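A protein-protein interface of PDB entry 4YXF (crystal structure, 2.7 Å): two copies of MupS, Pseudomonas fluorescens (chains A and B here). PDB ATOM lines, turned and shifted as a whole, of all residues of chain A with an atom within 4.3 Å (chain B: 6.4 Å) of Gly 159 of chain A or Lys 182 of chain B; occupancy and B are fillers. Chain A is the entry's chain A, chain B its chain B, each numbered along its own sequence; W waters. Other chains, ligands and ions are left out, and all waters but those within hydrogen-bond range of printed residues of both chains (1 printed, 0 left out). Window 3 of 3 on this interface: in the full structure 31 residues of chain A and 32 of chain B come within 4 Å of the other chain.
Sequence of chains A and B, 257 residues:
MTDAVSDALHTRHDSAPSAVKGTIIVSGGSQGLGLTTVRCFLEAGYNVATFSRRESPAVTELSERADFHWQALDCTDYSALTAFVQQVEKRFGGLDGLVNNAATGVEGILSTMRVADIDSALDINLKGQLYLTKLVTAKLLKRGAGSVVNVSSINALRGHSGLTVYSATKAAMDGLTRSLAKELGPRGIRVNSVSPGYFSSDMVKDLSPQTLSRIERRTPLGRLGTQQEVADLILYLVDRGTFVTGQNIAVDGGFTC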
ATOM      1  N   ASN A 155      -5.652  -9.993   5.511  1.00  0.00           N
ATOM      2  CA  ASN A 155      -5.616  -9.057   4.394  1.00  0.00           C
ATOM      3  C   ASN A 155      -5.482  -9.761   3.072  1.00  0.00           C
ATOM      4  O   ASN A 155      -5.747  -9.184   2.026  1.00  0.00           O
ATOM      5  CB  ASN A 155      -4.501  -8.025   4.503  1.00  0.00           C
ATOM      6  CG  ASN A 155      -4.571  -7.240   5.790  1.00  0.00           C
ATOM      7  OD1 ASN A 155      -5.666  -6.853   6.267  1.00  0.00           O
ATOM      8  ND2 ASN A 155      -3.398  -7.005   6.378  1.00  0.00           N
ATOM      9  N   LEU A 157      -7.229 -12.298   2.315  1.00  0.00           N
ATOM     10  CA  LEU A 157      -8.575 -12.778   2.036  1.00  0.00           C
ATOM     11  C   LEU A 157      -9.617 -11.683   1.916  1.00  0.00           C
ATOM     12  O   LEU A 157     -10.633 -11.923   1.291  1.00  0.00           O
ATOM     13  CB  LEU A 157      -9.063 -13.681   3.167  1.00  0.00           C
ATOM     14  CG  LEU A 157      -8.148 -14.836   3.534  1.00  0.00           C
ATOM     15  CD1 LEU A 157      -8.587 -15.553   4.796  1.00  0.00           C
ATOM     16  CD2 LEU A 157      -8.170 -15.753   2.360  1.00  0.00           C
ATOM     17  N   ARG A 158      -9.413 -10.528   2.507  1.00  0.00           N
ATOM     18  CA  ARG A 158     -10.452  -9.524   2.449  1.00  0.00           C
ATOM     19  C   ARG A 158     -10.123  -8.194   1.831  1.00  0.00           C
ATOM     20  O   ARG A 158     -10.840  -7.718   0.993  1.00  0.00           O
ATOM     21  CB  ARG A 158     -11.096  -9.312   3.787  1.00  0.00           C
ATOM     22  CG  ARG A 158     -11.865 -10.490   4.293  1.00  0.00           C
ATOM     23  CD  ARG A 158     -12.853 -11.024   3.302  1.00  0.00           C
ATOM     24  NE  ARG A 158     -13.559 -12.154   3.854  1.00  0.00           N
ATOM     25  CZ  ARG A 158     -13.711 -13.308   3.244  1.00  0.00           C
ATOM     26  NH1 ARG A 158     -13.221 -13.475   2.050  1.00  0.00           N
ATOM     27  NH2 ARG A 158     -14.362 -14.289   3.820  1.00  0.00           N
ATOM     28  N   GLY A 159      -9.068  -7.551   2.211  1.00  0.00           N
ATOM     29  CA  GLY A 159      -8.844  -6.308   1.530  1.00  0.00           C
ATOM     30  C   GLY A 159      -9.211  -5.113   2.349  1.00  0.00           C
ATOM     31  O   GLY A 159     -10.320  -4.950   2.794  1.00  0.00           O
ATOM     32  N   HIS A 160      -8.214  -4.280   2.535  1.00  0.00           N
ATOM     33  CA  HIS A 160      -8.191  -3.303   3.527  1.00  0.00           C
ATOM     34  C   HIS A 160      -7.512  -2.226   2.812  1.00  0.00           C
ATOM     35  O   HIS A 160      -6.482  -2.439   2.223  1.00  0.00           O
ATOM     36  CB  HIS A 160      -7.306  -3.829   4.631  1.00  0.00           C
ATOM     37  CG  HIS A 160      -7.321  -3.035   5.895  1.00  0.00           C
ATOM     38  ND1 HIS A 160      -6.950  -1.770   5.947  1.00  0.00           N
ATOM     39  CD2 HIS A 160      -7.627  -3.398   7.176  1.00  0.00           C
ATOM     40  CE1 HIS A 160      -7.035  -1.334   7.193  1.00  0.00           C
ATOM     41  NE2 HIS A 160      -7.448  -2.329   7.944  1.00  0.00           N
ATOM     42  N   SER A 161      -8.090  -1.051   2.820  1.00  0.00           N
ATOM     43  CA  SER A 161      -7.479   0.082   2.205  1.00  0.00           C
ATOM     44  C   SER A 161      -6.115   0.352   2.798  1.00  0.00           C
ATOM     45  O   SER A 161      -5.904   0.170   3.968  1.00  0.00           O
ATOM     46  CB  SER A 161      -8.381   1.253   2.417  1.00  0.00           C
ATOM     47  OG  SER A 161      -7.774   2.411   1.966  1.00  0.00           O
ATOM     48  N   GLY B 175      -4.975 -10.477  -4.672  1.00  0.00           N
ATOM     49  CA  GLY B 175      -5.000  -9.964  -3.338  1.00  0.00           C
ATOM     50  C   GLY B 175      -5.046  -8.465  -3.508  1.00  0.00           C
ATOM     51  O   GLY B 175      -5.717  -7.756  -2.768  1.00  0.00           O
ATOM     52  N   THR B 177      -6.325  -6.882  -6.196  1.00  0.00           N
ATOM     53  CA  THR B 177      -7.674  -6.527  -6.567  1.00  0.00           C
ATOM     54  C   THR B 177      -8.553  -6.206  -5.341  1.00  0.00           C
ATOM     55  O   THR B 177      -9.190  -5.126  -5.300  1.00  0.00           O
ATOM     56  CB  THR B 177      -8.363  -7.658  -7.339  1.00  0.00           C
ATOM     57  OG1 THR B 177      -7.775  -7.786  -8.638  1.00  0.00           O
ATOM     58  CG2 THR B 177      -9.919  -7.449  -7.460  1.00  0.00           C
ATOM     59  N   ARG B 178      -8.615  -7.143  -4.374  1.00  0.00           N
ATOM     60  CA  ARG B 178      -9.578  -7.008  -3.270  1.00  0.00           C
ATOM     61  C   ARG B 178      -9.231  -5.741  -2.520  1.00  0.00           C
ATOM     62  O   ARG B 178     -10.096  -4.919  -2.155  1.00  0.00           O
ATOM     63  CB  ARG B 178      -9.513  -8.202  -2.309  1.00  0.00           C
ATOM     64  CG  ARG B 178     -10.297  -9.376  -2.760  1.00  0.00           C
ATOM     65  CD  ARG B 178     -10.251 -10.496  -1.753  1.00  0.00           C
ATOM     66  NE  ARG B 178      -8.958 -11.152  -1.739  1.00  0.00           N
ATOM     67  CZ  ARG B 178      -8.499 -12.061  -2.624  1.00  0.00           C
ATOM     68  NH1 ARG B 178      -9.234 -12.480  -3.639  1.00  0.00           N
ATOM     69  NH2 ARG B 178      -7.267 -12.598  -2.450  1.00  0.00           N
ATOM     70  N   SER B 179      -7.931  -5.575  -2.327  1.00  0.00           N
ATOM     71  CA  SER B 179      -7.424  -4.444  -1.586  1.00  0.00           C
ATOM     72  C   SER B 179      -7.664  -3.104  -2.224  1.00  0.00           C
ATOM     73  O   SER B 179      -8.188  -2.196  -1.591  1.00  0.00           O
ATOM     74  CB  SER B 179      -5.941  -4.589  -1.426  1.00  0.00           C
ATOM     75  OG  SER B 179      -5.593  -3.758  -0.363  1.00  0.00           O
ATOM     76  N   LEU B 180      -7.211  -2.972  -3.464  1.00  0.00           N
ATOM     77  CA  LEU B 180      -7.366  -1.777  -4.252  1.00  0.00           C
ATOM     78  C   LEU B 180      -8.872  -1.459  -4.472  1.00  0.00           C
ATOM     79  O   LEU B 180      -9.282  -0.289  -4.492  1.00  0.00           O
ATOM     80  CB  LEU B 180      -6.665  -2.035  -5.549  1.00  0.00           C
ATOM     81  CG  LEU B 180      -6.319  -0.902  -6.440  1.00  0.00           C
ATOM     82  CD1 LEU B 180      -5.320  -0.046  -5.706  1.00  0.00           C
ATOM     83  CD2 LEU B 180      -5.650  -1.485  -7.645  1.00  0.00           C
ATOM     84  N   ALA B 181      -9.698  -2.482  -4.608  1.00  0.00           N
ATOM     85  CA  ALA B 181     -11.133  -2.252  -4.547  1.00  0.00           C
ATOM     86  C   ALA B 181     -11.577  -1.452  -3.299  1.00  0.00           C
ATOM     87  O   ALA B 181     -12.410  -0.548  -3.403  1.00  0.00           O
ATOM     88  CB  ALA B 181     -11.931  -3.564  -4.633  1.00  0.00           C
ATOM     89  N   LYS B 182     -11.066  -1.822  -2.131  1.00  0.00           N
ATOM     90  CA  LYS B 182     -11.447  -1.136  -0.899  1.00  0.00           C
ATOM     91  C   LYS B 182     -10.874   0.267  -0.921  1.00  0.00           C
ATOM     92  O   LYS B 182     -11.546   1.197  -0.539  1.00  0.00           O
ATOM     93  CB  LYS B 182     -10.970  -1.920   0.338  1.00  0.00           C
ATOM     94  CG  LYS B 182     -11.732  -1.630   1.631  1.00  0.00           C
ATOM     95  CD  LYS B 182     -13.007  -2.476   1.769  1.00  0.00           C
ATOM     96  CE  LYS B 182     -13.671  -2.373   3.165  1.00  0.00           C
ATOM     97  NZ  LYS B 182     -14.823  -1.439   3.244  1.00  0.00           N
ATOM     98  N   GLU B 183      -9.652   0.421  -1.420  1.00  0.00           N
ATOM     99  CA  GLU B 183      -8.996   1.720  -1.453  1.00  0.00           C
ATOM    100  C   GLU B 183      -9.541   2.748  -2.444  1.00  0.00           C
ATOM    101  O   GLU B 183      -9.622   3.891  -2.075  1.00  0.00           O
ATOM    102  CB  GLU B 183      -7.534   1.513  -1.753  1.00  0.00           C
ATOM    103  CG  GLU B 183      -6.625   2.744  -1.741  1.00  0.00           C
ATOM    104  CD  GLU B 183      -5.163   2.284  -1.634  1.00  0.00           C
ATOM    105  OE1 GLU B 183      -4.835   1.542  -0.675  1.00  0.00           O
ATOM    106  OE2 GLU B 183      -4.337   2.601  -2.518  1.00  0.00           O
ATOM    107  N   LEU B 184      -9.861   2.351  -3.682  1.00  0.00           N
ATOM    108  CA  LEU B 184     -10.154   3.254  -4.776  1.00  0.00           C
ATOM    109  C   LEU B 184     -11.661   3.359  -4.911  1.00  0.00           C
ATOM    110  O   LEU B 184     -12.232   4.177  -5.696  1.00  0.00           O
ATOM    111  CB  LEU B 184      -9.606   2.708  -6.074  1.00  0.00           C
ATOM    112  CG  LEU B 184      -8.090   2.703  -6.122  1.00  0.00           C
ATOM    113  CD1 LEU B 184      -7.638   2.379  -7.535  1.00  0.00           C
ATOM    114  CD2 LEU B 184      -7.534   4.023  -5.589  1.00  0.00           C
ATOM    115  N   GLY B 185     -12.316   2.560  -4.125  1.00  0.00           N
ATOM    116  CA  GLY B 185     -13.728   2.447  -4.230  1.00  0.00           C
ATOM    117  C   GLY B 185     -14.441   3.680  -3.844  1.00  0.00           C
ATOM    118  O   GLY B 185     -15.395   4.018  -4.459  1.00  0.00           O
ATOM    119  N   PRO B 186     -13.997   4.352  -2.812  1.00  0.00           N
ATOM    120  CA  PRO B 186     -14.722   5.552  -2.406  1.00  0.00           C
ATOM    121  C   PRO B 186     -14.413   6.691  -3.346  1.00  0.00           C
ATOM    122  O   PRO B 186     -14.981   7.750  -3.215  1.00  0.00           O
ATOM    123  CB  PRO B 186     -14.153   5.851  -1.033  1.00  0.00           C
ATOM    124  CG  PRO B 186     -13.620   4.537  -0.563  1.00  0.00           C
ATOM    125  CD  PRO B 186     -12.998   3.965  -1.801  1.00  0.00           C
ATOM    126  N   VAL B 191     -12.621  -2.354  -9.148  1.00  0.00           N
ATOM    127  CA  VAL B 191     -11.483  -3.182  -9.486  1.00  0.00           C
ATOM    128  C   VAL B 191     -11.898  -4.667  -9.393  1.00  0.00           C
ATOM    129  O   VAL B 191     -12.557  -5.055  -8.399  1.00  0.00           O
ATOM    130  CB  VAL B 191     -10.311  -2.922  -8.499  1.00  0.00           C
ATOM    131  CG1 VAL B 191      -9.044  -3.701  -8.911  1.00  0.00           C
ATOM    132  CG2 VAL B 191     -10.046  -1.444  -8.379  1.00  0.00           C
ATOM    133  N   THR B 245     -17.610  -4.917  -7.758  1.00  0.00           N
ATOM    134  CA  THR B 245     -16.220  -4.668  -7.549  1.00  0.00           C
ATOM    135  C   THR B 245     -15.696  -5.589  -6.466  1.00  0.00           C
ATOM    136  O   THR B 245     -16.436  -5.987  -5.552  1.00  0.00           O
ATOM    137  CB  THR B 245     -16.013  -3.213  -7.150  1.00  0.00           C
ATOM    138  OG1 THR B 245     -14.607  -2.875  -7.219  1.00  0.00           O
ATOM    139  CG2 THR B 245     -16.548  -3.032  -5.774  1.00  0.00           C
HETATM  140  O   HOH W   1      -6.928  -9.490  -0.480  1.00  0.00           O
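The side-chain hydroxyl of Ser 179 of chain B lies within hydrogen-bond range of the backbone carbonyl oxygen of His 160 of chain A, at 3.0 Å.
Of chain B, only Ser 179 and Lys 182 come within 4 Å of Gly 159 of chain A. Printed residues of chain A within 4 Å of Glu 183 of chain B: Ser 161 (3.7 Å). Of the printed residues of chain B, Arg 158 of chain A touches Arg 178. Printed residues of chain A within 4 Å of Ser 179 of chain B: Gly 159 and His 160. Of the printed residues of chain B, Ser 161 of chain A touches Lys 182 (3.9 Å) and Glu 183 (3.7 Å). The nearest residue of chain A that does not touch Lys 182 of chain B is His 160 of chain A (4.2 Å).
No position is printed for both chains.
Of the 13 printed residues of chain B, 4 touch a printed residue of chain A. Printed residues of chain B that touch a printed residue of chain A: Arg 178, Ser 179, Lys 182 and Glu 183. Among the printed residues, 7 pairs touch across the chains. Among the printed residues, no Asp or Glu carboxylate lies within 4 Å of a Lys or Arg side-chain nitrogen of the other chain.
Water W1 lies within hydrogen-bond range of O of Asn 155 of chain A (2.8 Å), NE of Arg 178 of chain B (2.9 Å) and O of Gly 175 of chain B (3.1 Å).
Among the printed residues, merely in contact across the chains: Leu 157 of chain A with Arg 178 of chain B, Arg 158 of chain A with Arg 178 of chain B, Ser 161 of chain A with Glu 183 of chain B, Gly 159 of chain A with Lys 182 of chain B, Ser 161 of chain A with Lys 182 of chain B and Gly 159 of chain A with Ser 179 of chain B.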
